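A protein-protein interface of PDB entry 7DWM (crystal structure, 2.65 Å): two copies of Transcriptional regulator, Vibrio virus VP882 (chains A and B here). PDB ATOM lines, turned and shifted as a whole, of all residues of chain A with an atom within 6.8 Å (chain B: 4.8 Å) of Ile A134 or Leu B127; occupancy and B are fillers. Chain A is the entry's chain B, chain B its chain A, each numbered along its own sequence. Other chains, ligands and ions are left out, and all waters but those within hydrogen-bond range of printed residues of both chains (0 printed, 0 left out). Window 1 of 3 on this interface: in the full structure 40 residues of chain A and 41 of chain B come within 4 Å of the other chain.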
ATOM      1  N   ASP A 129     -20.652 -11.490 -33.232  1.00  0.00           N
ATOM      2  CA  ASP A 129     -20.014 -10.538 -32.332  1.00  0.00           C
ATOM      3  C   ASP A 129     -19.491 -11.231 -31.079  1.00  0.00           C
ATOM      4  O   ASP A 129     -18.344 -11.012 -30.671  1.00  0.00           O
ATOM      5  CB  ASP A 129     -21.011  -9.432 -31.975  1.00  0.00           C
ATOM      6  CG  ASP A 129     -20.634  -8.682 -30.714  1.00  0.00           C
ATOM      7  OD1 ASP A 129     -21.010  -9.138 -29.613  1.00  0.00           O
ATOM      8  OD2 ASP A 129     -19.973  -7.629 -30.825  1.00  0.00           O
ATOM      9  N   THR A 130     -20.305 -12.089 -30.460  1.00  0.00           N
ATOM     10  CA  THR A 130     -19.837 -12.738 -29.242  1.00  0.00           C
ATOM     11  C   THR A 130     -18.807 -13.823 -29.542  1.00  0.00           C
ATOM     12  O   THR A 130     -17.915 -14.065 -28.719  1.00  0.00           O
ATOM     13  CB  THR A 130     -21.017 -13.319 -28.461  1.00  0.00           C
ATOM     14  OG1 THR A 130     -21.429 -14.557 -29.054  1.00  0.00           O
ATOM     15  CG2 THR A 130     -22.188 -12.343 -28.460  1.00  0.00           C
ATOM     16  N   ALA A 131     -18.866 -14.435 -30.729  1.00  0.00           N
ATOM     17  CA  ALA A 131     -17.806 -15.348 -31.151  1.00  0.00           C
ATOM     18  C   ALA A 131     -16.474 -14.617 -31.280  1.00  0.00           C
ATOM     19  O   ALA A 131     -15.441 -15.082 -30.780  1.00  0.00           O
ATOM     20  CB  ALA A 131     -18.187 -16.022 -32.468  1.00  0.00           C
ATOM     21  N   GLY A 132     -16.480 -13.463 -31.955  1.00  0.00           N
ATOM     22  CA  GLY A 132     -15.259 -12.682 -32.070  1.00  0.00           C
ATOM     23  C   GLY A 132     -14.755 -12.204 -30.723  1.00  0.00           C
ATOM     24  O   GLY A 132     -13.545 -12.139 -30.485  1.00  0.00           O
ATOM     25  N   ARG A 133     -15.680 -11.851 -29.826  1.00  0.00           N
ATOM     26  CA  ARG A 133     -15.292 -11.439 -28.482  1.00  0.00           C
ATOM     27  C   ARG A 133     -14.596 -12.579 -27.746  1.00  0.00           C
ATOM     28  O   ARG A 133     -13.559 -12.372 -27.103  1.00  0.00           O
ATOM     29  CB  ARG A 133     -16.519 -10.954 -27.709  1.00  0.00           C
ATOM     30  CG  ARG A 133     -16.747  -9.450 -27.800  1.00  0.00           C
ATOM     31  CD  ARG A 133     -18.211  -9.082 -27.610  1.00  0.00           C
ATOM     32  NE  ARG A 133     -18.368  -7.882 -26.792  1.00  0.00           N
ATOM     33  CZ  ARG A 133     -19.539  -7.348 -26.458  1.00  0.00           C
ATOM     34  NH1 ARG A 133     -20.668  -7.902 -26.878  1.00  0.00           N
ATOM     35  NH2 ARG A 133     -19.583  -6.255 -25.708  1.00  0.00           N
ATOM     36  N   ILE A 134     -15.145 -13.794 -27.845  1.00  0.00           N
ATOM     37  CA  ILE A 134     -14.519 -14.947 -27.204  1.00  0.00           C
ATOM     38  C   ILE A 134     -13.167 -15.243 -27.832  1.00  0.00           C
ATOM     39  O   ILE A 134     -12.232 -15.668 -27.140  1.00  0.00           O
ATOM     40  CB  ILE A 134     -15.455 -16.173 -27.301  1.00  0.00           C
ATOM     41  CG1 ILE A 134     -16.671 -16.003 -26.396  1.00  0.00           C
ATOM     42  CG2 ILE A 134     -14.712 -17.459 -26.958  1.00  0.00           C
ATOM     43  CD1 ILE A 134     -17.769 -16.992 -26.687  1.00  0.00           C
ATOM     44  N   GLU A 135     -13.010 -14.960 -29.125  1.00  0.00           N
ATOM     45  CA  GLU A 135     -11.719 -15.212 -29.759  1.00  0.00           C
ATOM     46  C   GLU A 135     -10.670 -14.216 -29.280  1.00  0.00           C
ATOM     47  O   GLU A 135      -9.523 -14.594 -29.014  1.00  0.00           O
ATOM     48  CB  GLU A 135     -11.851 -15.170 -31.281  1.00  0.00           C
ATOM     49  CG  GLU A 135     -10.700 -15.862 -31.999  1.00  0.00           C
ATOM     50  CD  GLU A 135     -10.467 -15.331 -33.398  1.00  0.00           C
ATOM     51  OE1 GLU A 135     -10.903 -15.992 -34.362  1.00  0.00           O
ATOM     52  OE2 GLU A 135      -9.845 -14.258 -33.534  1.00  0.00           O
ATOM     53  N   ARG A 136     -11.049 -12.942 -29.151  1.00  0.00           N
ATOM     54  CA  ARG A 136     -10.122 -11.952 -28.605  1.00  0.00           C
ATOM     55  C   ARG A 136      -9.779 -12.266 -27.152  1.00  0.00           C
ATOM     56  O   ARG A 136      -8.624 -12.106 -26.727  1.00  0.00           O
ATOM     57  CB  ARG A 136     -10.719 -10.552 -28.746  1.00  0.00           C
ATOM     58  CG  ARG A 136     -11.113 -10.208 -30.179  1.00  0.00           C
ATOM     59  CD  ARG A 136     -11.475  -8.740 -30.336  1.00  0.00           C
ATOM     60  NE  ARG A 136     -12.825  -8.570 -30.870  1.00  0.00           N
ATOM     61  CZ  ARG A 136     -13.912  -8.437 -30.117  1.00  0.00           C
ATOM     62  NH1 ARG A 136     -13.809  -8.446 -28.796  1.00  0.00           N
ATOM     63  NH2 ARG A 136     -15.102  -8.290 -30.684  1.00  0.00           N
ATOM     64  N   ALA A 137     -10.760 -12.752 -26.385  1.00  0.00           N
ATOM     65  CA  ALA A 137     -10.491 -13.180 -25.015  1.00  0.00           C
ATOM     66  C   ALA A 137      -9.490 -14.328 -24.984  1.00  0.00           C
ATOM     67  O   ALA A 137      -8.603 -14.361 -24.127  1.00  0.00           O
ATOM     68  CB  ALA A 137     -11.789 -13.581 -24.315  1.00  0.00           C
ATOM     69  N   VAL A 138      -9.642 -15.306 -25.882  1.00  0.00           N
ATOM     70  CA  VAL A 138      -8.708 -16.432 -25.926  1.00  0.00           C
ATOM     71  C   VAL A 138      -7.319 -15.968 -26.349  1.00  0.00           C
ATOM     72  O   VAL A 138      -6.299 -16.444 -25.825  1.00  0.00           O
ATOM     73  CB  VAL A 138      -9.243 -17.530 -26.862  1.00  0.00           C
ATOM     74  CG1 VAL A 138      -8.157 -18.543 -27.176  1.00  0.00           C
ATOM     75  CG2 VAL A 138     -10.455 -18.206 -26.244  1.00  0.00           C
ATOM     76  N   VAL A 139      -7.268 -14.987 -27.245  1.00  0.00           N
ATOM     77  CA  VAL A 139      -5.950 -14.446 -27.682  1.00  0.00           C
ATOM     78  C   VAL A 139      -5.287 -13.774 -26.479  1.00  0.00           C
ATOM     79  O   VAL A 139      -4.086 -13.976 -26.281  1.00  0.00           O
ATOM     80  CB  VAL A 139      -6.110 -13.455 -28.848  1.00  0.00           C
ATOM     81  CG1 VAL A 139      -4.785 -12.808 -29.211  1.00  0.00           C
ATOM     82  CG2 VAL A 139      -6.736 -14.120 -30.060  1.00  0.00           C
ATOM     83  N   VAL B 102     -17.420 -24.151 -19.644  1.00  0.00           N
ATOM     84  CA  VAL B 102     -17.167 -22.868 -20.284  1.00  0.00           C
ATOM     85  C   VAL B 102     -18.516 -22.169 -20.374  1.00  0.00           C
ATOM     86  O   VAL B 102     -19.320 -22.465 -21.264  1.00  0.00           O
ATOM     87  CB  VAL B 102     -16.535 -23.036 -21.671  1.00  0.00           C
ATOM     88  CG1 VAL B 102     -16.237 -21.681 -22.294  1.00  0.00           C
ATOM     89  CG2 VAL B 102     -15.276 -23.891 -21.591  1.00  0.00           C
ATOM     90  N   PHE B 103     -18.791 -21.260 -19.447  1.00  0.00           N
ATOM     91  CA  PHE B 103     -20.033 -20.514 -19.470  1.00  0.00           C
ATOM     92  C   PHE B 103     -19.803 -19.105 -19.992  1.00  0.00           C
ATOM     93  O   PHE B 103     -18.708 -18.545 -19.910  1.00  0.00           O
ATOM     94  CB  PHE B 103     -20.657 -20.449 -18.074  1.00  0.00           C
ATOM     95  CG  PHE B 103     -21.709 -21.486 -17.837  1.00  0.00           C
ATOM     96  CD1 PHE B 103     -23.032 -21.119 -17.649  1.00  0.00           C
ATOM     97  CD2 PHE B 103     -21.380 -22.829 -17.802  1.00  0.00           C
ATOM     98  CE1 PHE B 103     -24.006 -22.075 -17.430  1.00  0.00           C
ATOM     99  CE2 PHE B 103     -22.350 -23.791 -17.584  1.00  0.00           C
ATOM    100  CZ  PHE B 103     -23.664 -23.412 -17.397  1.00  0.00           C
ATOM    101  N   THR B 104     -20.871 -18.543 -20.535  1.00  0.00           N
ATOM    102  CA  THR B 104     -21.009 -17.113 -20.748  1.00  0.00           C
ATOM    103  C   THR B 104     -21.990 -16.590 -19.709  1.00  0.00           C
ATOM    104  O   THR B 104     -23.131 -17.060 -19.643  1.00  0.00           O
ATOM    105  CB  THR B 104     -21.498 -16.845 -22.172  1.00  0.00           C
ATOM    106  OG1 THR B 104     -20.427 -17.075 -23.099  1.00  0.00           O
ATOM    107  CG2 THR B 104     -22.065 -15.442 -22.327  1.00  0.00           C
ATOM    108  N   GLN B 125     -24.958 -18.942 -19.708  1.00  0.00           N
ATOM    109  CA  GLN B 125     -25.219 -19.835 -20.833  1.00  0.00           C
ATOM    110  C   GLN B 125     -24.087 -20.844 -20.967  1.00  0.00           C
ATOM    111  O   GLN B 125     -22.915 -20.463 -21.045  1.00  0.00           O
ATOM    112  CB  GLN B 125     -25.375 -19.047 -22.139  1.00  0.00           C
ATOM    113  CG  GLN B 125     -26.320 -17.859 -22.048  1.00  0.00           C
ATOM    114  CD  GLN B 125     -26.776 -17.377 -23.410  1.00  0.00           C
ATOM    115  OE1 GLN B 125     -26.629 -16.203 -23.748  1.00  0.00           O
ATOM    116  NE2 GLN B 125     -27.335 -18.286 -24.203  1.00  0.00           N
ATOM    117  N   ASP B 126     -24.448 -22.128 -21.002  1.00  0.00           N
ATOM    118  CA  ASP B 126     -23.477 -23.211 -21.124  1.00  0.00           C
ATOM    119  C   ASP B 126     -23.016 -23.324 -22.571  1.00  0.00           C
ATOM    120  O   ASP B 126     -23.764 -23.781 -23.441  1.00  0.00           O
ATOM    121  CB  ASP B 126     -24.084 -24.526 -20.642  1.00  0.00           C
ATOM    122  CG  ASP B 126     -23.045 -25.621 -20.480  1.00  0.00           C
ATOM    123  OD1 ASP B 126     -23.432 -26.762 -20.150  1.00  0.00           O
ATOM    124  OD2 ASP B 126     -21.843 -25.344 -20.681  1.00  0.00           O
ATOM    125  N   LEU B 127     -21.777 -22.914 -22.825  1.00  0.00           N
ATOM    126  CA  LEU B 127     -21.217 -22.885 -24.168  1.00  0.00           C
ATOM    127  C   LEU B 127     -20.611 -24.210 -24.617  1.00  0.00           C
ATOM    128  O   LEU B 127     -20.383 -24.383 -25.817  1.00  0.00           O
ATOM    129  CB  LEU B 127     -20.164 -21.780 -24.274  1.00  0.00           C
ATOM    130  CG  LEU B 127     -20.738 -20.363 -24.293  1.00  0.00           C
ATOM    131  CD1 LEU B 127     -19.775 -19.424 -24.988  1.00  0.00           C
ATOM    132  CD2 LEU B 127     -22.106 -20.330 -24.969  1.00  0.00           C
ATOM    133  N   THR B 128     -20.331 -25.136 -23.695  1.00  0.00           N
ATOM    134  CA  THR B 128     -19.563 -26.332 -24.040  1.00  0.00           C
ATOM    135  C   THR B 128     -20.252 -27.184 -25.107  1.00  0.00           C
ATOM    136  O   THR B 128     -19.663 -27.482 -26.152  1.00  0.00           O
ATOM    137  CB  THR B 128     -19.325 -27.164 -22.778  1.00  0.00           C
ATOM    138  OG1 THR B 128     -20.582 -27.644 -22.286  1.00  0.00           O
ATOM    139  CG2 THR B 128     -18.667 -26.321 -21.698  1.00  0.00           C
ATOM    140  N   ASP B 129     -21.495 -27.600 -24.859  1.00  0.00           N
ATOM    141  CA  ASP B 129     -22.198 -28.457 -25.815  1.00  0.00           C
ATOM    142  C   ASP B 129     -22.665 -27.674 -27.041  1.00  0.00           C
ATOM    143  O   ASP B 129     -22.541 -28.139 -28.190  1.00  0.00           O
ATOM    144  CB  ASP B 129     -23.380 -29.149 -25.132  1.00  0.00           C
ATOM    145  CG  ASP B 129     -24.390 -28.165 -24.570  1.00  0.00           C
ATOM    146  OD1 ASP B 129     -23.986 -27.037 -24.214  1.00  0.00           O
ATOM    147  OD2 ASP B 129     -25.585 -28.520 -24.487  1.00  0.00           O
ATOM    148  N   THR B 130     -23.208 -26.481 -26.811  1.00  0.00           N
ATOM    149  CA  THR B 130     -23.781 -25.717 -27.904  1.00  0.00           C
ATOM    150  C   THR B 130     -22.718 -25.186 -28.850  1.00  0.00           C
ATOM    151  O   THR B 130     -23.022 -24.961 -30.021  1.00  0.00           O
ATOM    152  CB  THR B 130     -24.624 -24.566 -27.358  1.00  0.00           C
ATOM    153  OG1 THR B 130     -23.775 -23.620 -26.698  1.00  0.00           O
ATOM    154  CG2 THR B 130     -25.659 -25.089 -26.371  1.00  0.00           C
ATOM    155  N   ALA B 131     -21.472 -25.040 -28.398  1.00  0.00           N
ATOM    156  CA  ALA B 131     -20.405 -24.670 -29.319  1.00  0.00           C
ATOM    157  C   ALA B 131     -20.269 -25.705 -30.428  1.00  0.00           C
ATOM    158  O   ALA B 131     -20.282 -25.364 -31.615  1.00  0.00           O
ATOM    159  CB  ALA B 131     -19.088 -24.508 -28.556  1.00  0.00           C
ATOM    160  N   LEU B 237     -15.835  -9.739 -21.972  1.00  0.00           N
ATOM    161  CA  LEU B 237     -15.583  -9.716 -23.400  1.00  0.00           C
ATOM    162  C   LEU B 237     -15.697  -8.295 -23.927  1.00  0.00           C
ATOM    163  O   LEU B 237     -16.565  -7.526 -23.506  1.00  0.00           O
ATOM    164  CB  LEU B 237     -16.537 -10.671 -24.109  1.00  0.00           C
ATOM    165  CG  LEU B 237     -16.279 -12.067 -23.528  1.00  0.00           C
ATOM    166  CD1 LEU B 237     -17.551 -12.856 -23.317  1.00  0.00           C
ATOM    167  CD2 LEU B 237     -15.306 -12.845 -24.388  1.00  0.00           C
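Of the 11 printed residues of chain A, 3 touch a printed residue of chain B.
Hydrophobic or aromatic side chains of chain A within 4 Å of the printed part of chain B: Ile A134 and Ala A137.
Of the 11 printed residues of chain B, 2 touch a printed residue of chain A.
Among the printed residues, 4 pairs touch across the chains.
Arg A133 touches Leu B237 (O to CD2, 3.3 Å).
CD1 of Ile A134 touches CD1 of Leu B127 (3.6 Å).
Ile A134 touches Leu B237.
CB of Ala A137 touches CD2 of Leu B237, 3.6 Å away.
Of the printed residues of chain B, Arg A133 touches Leu B237 (3.3 Å).
Of the printed residues of chain B, Ala A137 touches Leu B237.
Gln B125 touches none of the printed residues of chain A.
Printed residues of chain A within 4 Å of Leu B127: Ile A134.
Thr B130 touches none of the printed residues of chain A.
Printed residues of chain A within 4 Å of Leu B237: Arg A133 (3.3 Å), Ile A134 (3.6 Å) and Ala A137 (3.6 Å).
The nearest residue of chain A that does not touch Leu B127 is Thr A130 (6.6 Å).
NH1 of Arg A133 lies within salt-bridge range of OD1 of Asp A129 (3.0 Å).
O of Val B102 lies within hydrogen-bond range of N of Leu B127.
Positions printed for both chains: 129, 130 and 131.
Of the 4 pairs that touch across the chains among the printed residues, none has its exchanged pair printed and touching as well.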
